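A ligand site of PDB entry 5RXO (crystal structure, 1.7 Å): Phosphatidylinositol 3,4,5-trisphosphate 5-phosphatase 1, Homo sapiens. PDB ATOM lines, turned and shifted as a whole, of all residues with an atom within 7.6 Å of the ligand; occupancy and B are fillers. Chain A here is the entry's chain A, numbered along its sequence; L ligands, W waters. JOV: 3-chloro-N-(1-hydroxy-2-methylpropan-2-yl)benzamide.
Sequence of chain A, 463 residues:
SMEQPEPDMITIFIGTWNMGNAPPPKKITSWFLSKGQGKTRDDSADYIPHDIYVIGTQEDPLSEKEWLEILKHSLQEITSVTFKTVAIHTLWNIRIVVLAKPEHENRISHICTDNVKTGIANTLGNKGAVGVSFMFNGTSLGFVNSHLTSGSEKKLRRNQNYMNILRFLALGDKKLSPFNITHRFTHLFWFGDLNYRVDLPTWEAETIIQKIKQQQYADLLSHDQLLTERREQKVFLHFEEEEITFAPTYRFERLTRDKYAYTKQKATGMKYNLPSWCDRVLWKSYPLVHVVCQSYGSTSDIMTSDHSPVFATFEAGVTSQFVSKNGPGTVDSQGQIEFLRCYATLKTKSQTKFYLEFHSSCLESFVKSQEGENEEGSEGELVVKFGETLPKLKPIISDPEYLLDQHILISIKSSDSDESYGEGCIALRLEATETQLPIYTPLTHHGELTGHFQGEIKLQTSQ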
ATOM      1  N   LEU A  68      -0.069   9.785  31.808  1.00  0.00           N
ATOM      2  CA  LEU A  68      -1.469  10.267  31.849  1.00  0.00           C
ATOM      3  C   LEU A  68      -1.723  11.201  33.046  1.00  0.00           C
ATOM      4  O   LEU A  68      -2.412  12.233  32.871  1.00  0.00           O
ATOM      5  CB  LEU A  68      -2.440   9.097  31.856  1.00  0.00           C
ATOM      6  CG  LEU A  68      -2.645   8.456  30.498  1.00  0.00           C
ATOM      7  CD1 LEU A  68      -3.372   7.136  30.641  1.00  0.00           C
ATOM      8  CD2 LEU A  68      -3.420   9.406  29.599  1.00  0.00           C
ATOM      9  N   PHE A  83      -9.739  16.560  31.037  1.00  0.00           N
ATOM     10  CA  PHE A  83      -9.789  15.964  29.675  1.00  0.00           C
ATOM     11  C   PHE A  83     -10.139  14.484  29.749  1.00  0.00           C
ATOM     12  O   PHE A  83      -9.749  13.793  30.684  1.00  0.00           O
ATOM     13  CB  PHE A  83      -8.475  16.272  28.947  1.00  0.00           C
ATOM     14  CG  PHE A  83      -8.479  17.641  28.345  1.00  0.00           C
ATOM     15  CD1 PHE A  83      -8.260  18.761  29.115  1.00  0.00           C
ATOM     16  CD2 PHE A  83      -8.753  17.811  27.001  1.00  0.00           C
ATOM     17  CE1 PHE A  83      -8.346  20.028  28.564  1.00  0.00           C
ATOM     18  CE2 PHE A  83      -8.801  19.077  26.443  1.00  0.00           C
ATOM     19  CZ  PHE A  83      -8.593  20.179  27.221  1.00  0.00           C
ATOM     20  N   LYS A  84     -10.851  13.989  28.744  1.00  0.00           N
ATOM     21  CA  LYS A  84     -11.141  12.544  28.578  1.00  0.00           C
ATOM     22  C   LYS A  84      -9.997  11.921  27.791  1.00  0.00           C
ATOM     23  O   LYS A  84      -9.484  12.584  26.842  1.00  0.00           O
ATOM     24  CB  LYS A  84     -12.423  12.327  27.781  1.00  0.00           C
ATOM     25  CG  LYS A  84     -13.643  12.928  28.463  1.00  0.00           C
ATOM     26  CD  LYS A  84     -14.042  12.119  29.688  1.00  0.00           C
ATOM     27  CE  LYS A  84     -15.303  12.639  30.349  1.00  0.00           C
ATOM     28  NZ  LYS A  84     -15.674  11.722  31.454  1.00  0.00           N
ATOM     29  N   THR A  85      -9.645  10.685  28.125  1.00  0.00           N
ATOM     30  CA  THR A  85      -8.627   9.922  27.383  1.00  0.00           C
ATOM     31  C   THR A  85      -9.297   9.232  26.206  1.00  0.00           C
ATOM     32  O   THR A  85     -10.065   8.312  26.418  1.00  0.00           O
ATOM     33  CB  THR A  85      -7.891   8.961  28.310  1.00  0.00           C
ATOM     34  OG1 THR A  85      -7.336   9.682  29.405  1.00  0.00           O
ATOM     35  CG2 THR A  85      -6.813   8.233  27.536  1.00  0.00           C
ATOM     36  N   VAL A  86      -8.965   9.652  24.984  1.00  0.00           N
ATOM     37  CA  VAL A  86      -9.483   9.054  23.721  1.00  0.00           C
ATOM     38  C   VAL A  86      -8.744   7.755  23.472  1.00  0.00           C
ATOM     39  O   VAL A  86      -9.394   6.697  23.179  1.00  0.00           O
ATOM     40  CB  VAL A  86      -9.334  10.016  22.532  1.00  0.00           C
ATOM     41  CG1 VAL A  86      -9.692   9.327  21.223  1.00  0.00           C
ATOM     42  CG2 VAL A  86     -10.153  11.280  22.728  1.00  0.00           C
ATOM     43  N   ALA A  87      -7.416   7.816  23.552  1.00  0.00           N
ATOM     44  CA  ALA A  87      -6.549   6.670  23.213  1.00  0.00           C
ATOM     45  C   ALA A  87      -5.147   6.871  23.779  1.00  0.00           C
ATOM     46  O   ALA A  87      -4.697   8.022  23.948  1.00  0.00           O
ATOM     47  CB  ALA A  87      -6.456   6.508  21.712  1.00  0.00           C
ATOM     48  N   ILE A  88      -4.484   5.770  24.036  1.00  0.00           N
ATOM     49  CA  ILE A  88      -3.041   5.748  24.387  1.00  0.00           C
ATOM     50  C   ILE A  88      -2.467   4.456  23.819  1.00  0.00           C
ATOM     51  O   ILE A  88      -3.179   3.401  23.848  1.00  0.00           O
ATOM     52  CB  ILE A  88      -2.836   5.897  25.904  1.00  0.00           C
ATOM     53  CG1 ILE A  88      -1.362   5.970  26.261  1.00  0.00           C
ATOM     54  CG2 ILE A  88      -3.529   4.796  26.684  1.00  0.00           C
ATOM     55  CD1 ILE A  88      -1.136   6.539  27.644  1.00  0.00           C
ATOM     56  N   VAL A  98      -3.954  10.646  23.108  1.00  0.00           N
ATOM     57  CA  VAL A  98      -5.003  11.569  22.597  1.00  0.00           C
ATOM     58  C   VAL A  98      -5.980  11.889  23.729  1.00  0.00           C
ATOM     59  O   VAL A  98      -6.606  10.948  24.251  1.00  0.00           O
ATOM     60  CB  VAL A  98      -5.736  11.029  21.370  1.00  0.00           C
ATOM     61  CG1 VAL A  98      -6.788  12.026  20.873  1.00  0.00           C
ATOM     62  CG2 VAL A  98      -4.737  10.678  20.293  1.00  0.00           C
ATOM     63  N   LEU A  99      -6.104  13.186  24.038  1.00  0.00           N
ATOM     64  CA  LEU A  99      -7.035  13.717  25.052  1.00  0.00           C
ATOM     65  C   LEU A  99      -8.026  14.644  24.336  1.00  0.00           C
ATOM     66  O   LEU A  99      -7.652  15.341  23.392  1.00  0.00           O
ATOM     67  CB  LEU A  99      -6.248  14.458  26.133  1.00  0.00           C
ATOM     68  CG  LEU A  99      -5.085  13.691  26.766  1.00  0.00           C
ATOM     69  CD1 LEU A  99      -4.409  14.566  27.789  1.00  0.00           C
ATOM     70  CD2 LEU A  99      -5.543  12.386  27.399  1.00  0.00           C
ATOM     71  N   ALA A 100      -9.255  14.710  24.830  1.00  0.00           N
ATOM     72  CA  ALA A 100     -10.290  15.591  24.231  1.00  0.00           C
ATOM     73  C   ALA A 100     -11.134  16.217  25.327  1.00  0.00           C
ATOM     74  O   ALA A 100     -11.294  15.644  26.405  1.00  0.00           O
ATOM     75  CB  ALA A 100     -11.155  14.794  23.307  1.00  0.00           C
ATOM     76  N   LYS A 101     -11.680  17.407  25.058  1.00  0.00           N
ATOM     77  CA  LYS A 101     -12.618  18.082  25.992  1.00  0.00           C
ATOM     78  C   LYS A 101     -13.825  17.178  26.194  1.00  0.00           C
ATOM     79  O   LYS A 101     -14.266  16.518  25.250  1.00  0.00           O
ATOM     80  CB  LYS A 101     -13.039  19.447  25.445  1.00  0.00           C
ATOM     81  CG  LYS A 101     -11.881  20.391  25.176  1.00  0.00           C
ATOM     82  CD  LYS A 101     -12.353  21.709  24.633  1.00  0.00           C
ATOM     83  CE  LYS A 101     -13.357  22.408  25.527  1.00  0.00           C
ATOM     84  NZ  LYS A 101     -14.004  23.518  24.798  1.00  0.00           N
ATOM     85  N   PRO A 102     -14.375  17.102  27.427  1.00  0.00           N
ATOM     86  CA  PRO A 102     -15.514  16.244  27.719  1.00  0.00           C
ATOM     87  C   PRO A 102     -16.709  16.416  26.796  1.00  0.00           C
ATOM     88  O   PRO A 102     -17.359  15.431  26.509  1.00  0.00           O
ATOM     89  CB  PRO A 102     -15.938  16.612  29.142  1.00  0.00           C
ATOM     90  CG  PRO A 102     -14.842  17.492  29.688  1.00  0.00           C
ATOM     91  CD  PRO A 102     -13.900  17.866  28.583  1.00  0.00           C
ATOM     92  N   HIS A 104     -16.728  16.581  23.788  1.00  0.00           N
ATOM     93  CA  HIS A 104     -16.473  15.828  22.522  1.00  0.00           C
ATOM     94  C   HIS A 104     -16.578  14.327  22.699  1.00  0.00           C
ATOM     95  O   HIS A 104     -16.445  13.580  21.686  1.00  0.00           O
ATOM     96  CB  HIS A 104     -15.108  16.215  21.972  1.00  0.00           C
ATOM     97  CG  HIS A 104     -15.057  17.651  21.582  1.00  0.00           C
ATOM     98  ND1 HIS A 104     -16.179  18.341  21.157  1.00  0.00           N
ATOM     99  CD2 HIS A 104     -14.028  18.518  21.570  1.00  0.00           C
ATOM    100  CE1 HIS A 104     -15.816  19.576  20.838  1.00  0.00           C
ATOM    101  NE2 HIS A 104     -14.489  19.713  21.085  1.00  0.00           N
ATOM    102  N   GLU A 105     -16.781  13.854  23.924  1.00  0.00           N
ATOM    103  CA  GLU A 105     -16.771  12.395  24.210  1.00  0.00           C
ATOM    104  C   GLU A 105     -17.693  11.617  23.250  1.00  0.00           C
ATOM    105  O   GLU A 105     -17.280  10.586  22.702  1.00  0.00           O
ATOM    106  CB  GLU A 105     -17.173  12.133  25.661  1.00  0.00           C
ATOM    107  CG  GLU A 105     -17.236  10.665  25.950  1.00  0.00           C
ATOM    108  CD  GLU A 105     -17.559  10.315  27.386  1.00  0.00           C
ATOM    109  OE1 GLU A 105     -17.541  11.223  28.210  1.00  0.00           O
ATOM    110  OE2 GLU A 105     -17.835   9.117  27.641  1.00  0.00           O
ATOM    111  N   ASN A 106     -18.895  12.143  23.033  1.00  0.00           N
ATOM    112  CA  ASN A 106     -19.976  11.460  22.271  1.00  0.00           C
ATOM    113  C   ASN A 106     -19.946  11.917  20.802  1.00  0.00           C
ATOM    114  O   ASN A 106     -20.892  11.577  20.056  1.00  0.00           O
ATOM    115  CB  ASN A 106     -21.298  11.638  23.010  1.00  0.00           C
ATOM    116  CG  ASN A 106     -21.253  10.942  24.356  1.00  0.00           C
ATOM    117  OD1 ASN A 106     -21.249   9.717  24.425  1.00  0.00           O
ATOM    118  ND2 ASN A 106     -21.180  11.704  25.432  1.00  0.00           N
ATOM    119  N   ARG A 107     -18.902  12.663  20.403  1.00  0.00           N
ATOM    120  CA  ARG A 107     -18.650  13.025  18.980  1.00  0.00           C
ATOM    121  C   ARG A 107     -17.544  12.118  18.417  1.00  0.00           C
ATOM    122  O   ARG A 107     -17.403  12.041  17.211  1.00  0.00           O
ATOM    123  CB  ARG A 107     -18.231  14.495  18.849  1.00  0.00           C
ATOM    124  CG  ARG A 107     -19.302  15.458  19.324  1.00  0.00           C
ATOM    125  CD  ARG A 107     -18.791  16.878  19.204  1.00  0.00           C
ATOM    126  NE  ARG A 107     -19.914  17.785  19.260  1.00  0.00           N
ATOM    127  CZ  ARG A 107     -20.012  18.838  20.046  1.00  0.00           C
ATOM    128  NH1 ARG A 107     -19.014  19.201  20.822  1.00  0.00           N
ATOM    129  NH2 ARG A 107     -21.111  19.575  19.996  1.00  0.00           N
ATOM    130  N   ILE A 108     -16.847  11.415  19.296  1.00  0.00           N
ATOM    131  CA  ILE A 108     -15.657  10.585  18.967  1.00  0.00           C
ATOM    132  C   ILE A 108     -16.042   9.098  18.983  1.00  0.00           C
ATOM    133  O   ILE A 108     -16.669   8.650  19.943  1.00  0.00           O
ATOM    134  CB  ILE A 108     -14.508  10.942  19.915  1.00  0.00           C
ATOM    135  CG1 ILE A 108     -14.046  12.375  19.632  1.00  0.00           C
ATOM    136  CG2 ILE A 108     -13.387   9.921  19.824  1.00  0.00           C
ATOM    137  CD1 ILE A 108     -13.170  12.982  20.717  1.00  0.00           C
ATOM    138  N   SER A 109     -15.709   8.384  17.909  1.00  0.00           N
ATOM    139  CA  SER A 109     -16.021   6.948  17.723  1.00  0.00           C
ATOM    140  C   SER A 109     -14.972   6.320  16.809  1.00  0.00           C
ATOM    141  O   SER A 109     -14.105   7.046  16.274  1.00  0.00           O
ATOM    142  CB  SER A 109     -17.415   6.777  17.136  1.00  0.00           C
ATOM    143  OG  SER A 109     -17.441   7.225  15.786  1.00  0.00           O
ATOM    144  N   HIS A 110     -15.035   5.003  16.620  1.00  0.00           N
ATOM    145  CA  HIS A 110     -14.151   4.262  15.679  1.00  0.00           C
ATOM    146  C   HIS A 110     -12.679   4.527  16.008  1.00  0.00           C
ATOM    147  O   HIS A 110     -11.841   4.756  15.100  1.00  0.00           O
ATOM    148  CB  HIS A 110     -14.485   4.635  14.239  1.00  0.00           C
ATOM    149  CG  HIS A 110     -15.857   4.227  13.833  1.00  0.00           C
ATOM    150  ND1 HIS A 110     -16.947   5.032  14.020  1.00  0.00           N
ATOM    151  CD2 HIS A 110     -16.325   3.115  13.241  1.00  0.00           C
ATOM    152  CE1 HIS A 110     -18.017   4.457  13.525  1.00  0.00           C
ATOM    153  NE2 HIS A 110     -17.659   3.293  13.052  1.00  0.00           N
ATOM    154  N   ILE A 111     -12.347   4.436  17.283  1.00  0.00           N
ATOM    155  CA  ILE A 111     -10.953   4.635  17.737  1.00  0.00           C
ATOM    156  C   ILE A 111     -10.142   3.406  17.328  1.00  0.00           C
ATOM    157  O   ILE A 111     -10.536   2.232  17.662  1.00  0.00           O
ATOM    158  CB  ILE A 111     -10.922   4.894  19.239  1.00  0.00           C
ATOM    159  CG1 ILE A 111     -11.667   6.179  19.595  1.00  0.00           C
ATOM    160  CG2 ILE A 111      -9.473   4.892  19.776  1.00  0.00           C
ATOM    161  CD1 ILE A 111     -12.117   6.196  21.036  1.00  0.00           C
ATOM    162  N   CYS A 112      -9.041   3.635  16.605  1.00  0.00           N
ATOM    163  CA  CYS A 112      -8.051   2.610  16.209  1.00  0.00           C
ATOM    164  C   CYS A 112      -6.673   3.010  16.727  1.00  0.00           C
ATOM    165  O   CYS A 112      -6.396   4.234  16.775  1.00  0.00           O
ATOM    166  CB  CYS A 112      -7.977   2.434  14.691  1.00  0.00           C
ATOM    167  SG  CYS A 112      -9.565   1.987  13.937  1.00  0.00           S
ATOM    168  N   THR A 113      -5.869   2.025  17.120  1.00  0.00           N
ATOM    169  CA  THR A 113      -4.457   2.230  17.538  1.00  0.00           C
ATOM    170  C   THR A 113      -3.668   1.138  16.847  1.00  0.00           C
ATOM    171  O   THR A 113      -4.212   0.032  16.614  1.00  0.00           O
ATOM    172  CB  THR A 113      -4.255   2.190  19.069  1.00  0.00           C
ATOM    173  OG1 THR A 113      -4.634   0.898  19.561  1.00  0.00           O
ATOM    174  CG2 THR A 113      -5.099   3.203  19.798  1.00  0.00           C
ATOM    175  N   VAL A 132      -2.909   6.622  16.161  1.00  0.00           N
ATOM    176  CA  VAL A 132      -4.328   6.627  16.570  1.00  0.00           C
ATOM    177  C   VAL A 132      -5.133   7.211  15.427  1.00  0.00           C
ATOM    178  O   VAL A 132      -4.719   8.265  14.851  1.00  0.00           O
ATOM    179  CB  VAL A 132      -4.561   7.446  17.839  1.00  0.00           C
ATOM    180  CG1 VAL A 132      -6.031   7.492  18.213  1.00  0.00           C
ATOM    181  CG2 VAL A 132      -3.740   6.910  18.984  1.00  0.00           C
HETATM  182  C10 JOV L   1     -14.261   6.194  23.435  1.00  0.00           C
HETATM  183  C13 JOV L   1     -13.679   8.797  24.182  1.00  0.00           C
HETATM  184  C01 JOV L   1     -11.128   3.715  27.112  1.00  0.00           C
HETATM  185  C02 JOV L   1     -10.288   4.467  26.064  1.00  0.00           C
HETATM  186  C03 JOV L   1      -9.045   5.093  26.724  1.00  0.00           C
HETATM  187  C04 JOV L   1      -9.809   3.473  25.008  1.00  0.00           C
HETATM  188  O05 JOV L   1      -9.087   4.124  23.995  1.00  0.00           O
HETATM  189  N06 JOV L   1     -11.117   5.542  25.512  1.00  0.00           N
HETATM  190  C07 JOV L   1     -12.379   5.302  24.833  1.00  0.00           C
HETATM  191  O08 JOV L   1     -12.800   4.194  24.684  1.00  0.00           O
HETATM  192  C09 JOV L   1     -13.203   6.449  24.300  1.00  0.00           C
HETATM  193  C11 JOV L   1     -15.027   7.246  22.956  1.00  0.00           C
HETATM  194  C12 JOV L   1     -14.729   8.540  23.321  1.00  0.00           C
HETATM  195  C14 JOV L   1     -12.918   7.757  24.680  1.00  0.00           C
HETATM  196 CL15 JOV L   1     -13.319  10.465  24.673  1.00  0.00          CL
HETATM  197  O   HOH W   1      -9.059   1.578  21.815  1.00  0.00           O
HETATM  198  O   HOH W   2      -6.299   3.349  23.805  1.00  0.00           O
HETATM  199  O   HOH W   3     -18.314   8.037  22.318  1.00  0.00           O
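O of Thr 85 sits at hydrogen-bond distance from N06 of the ligand, 3.1 Å away. The backbone carbonyl oxygen (O) of Val 86 is in hydrogen-bond range of an oxygen (O05) of the ligand (2.7 Å).
O of Val 98 is in hydrogen-bond range of N of Val 86, at 2.8 Å. OE1 of Glu 105 is in salt-bridge range of NZ of Lys 84 (3.8 Å). The backbone NH (N) of Lys 84 sits at hydrogen-bond distance from the backbone carbonyl oxygen (O) of Ala 100 (2.9 Å). The backbone carbonyl oxygen (O) of Ala 87 sits at hydrogen-bond distance from the backbone NH (N) of Val 98 (2.9 Å).
Lys 84 touches the ligand. CA of Ala 87 touches O05 of the ligand, 3.7 Å away. O of Glu 105 touches C12 of the ligand, at 3.3 Å. O of Ile 108 touches C11 of the ligand, at 3.7 Å. Ile 111 touches the ligand (CD1 to C10, 3.2 Å). Hydrophobic or aromatic side chains that line the ligand: Val 86, Ile 108 and Ile 111. Seven residues have an atom within 4 Å of the ligand: Lys 84, Thr 85, Val 86, Ala 87, Glu 105, Ile 108 and Ile 111.
Water W2 bridges an oxygen (O05) of the ligand (2.9 Å) and the backbone NH of Ile 88 (3.0 Å).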
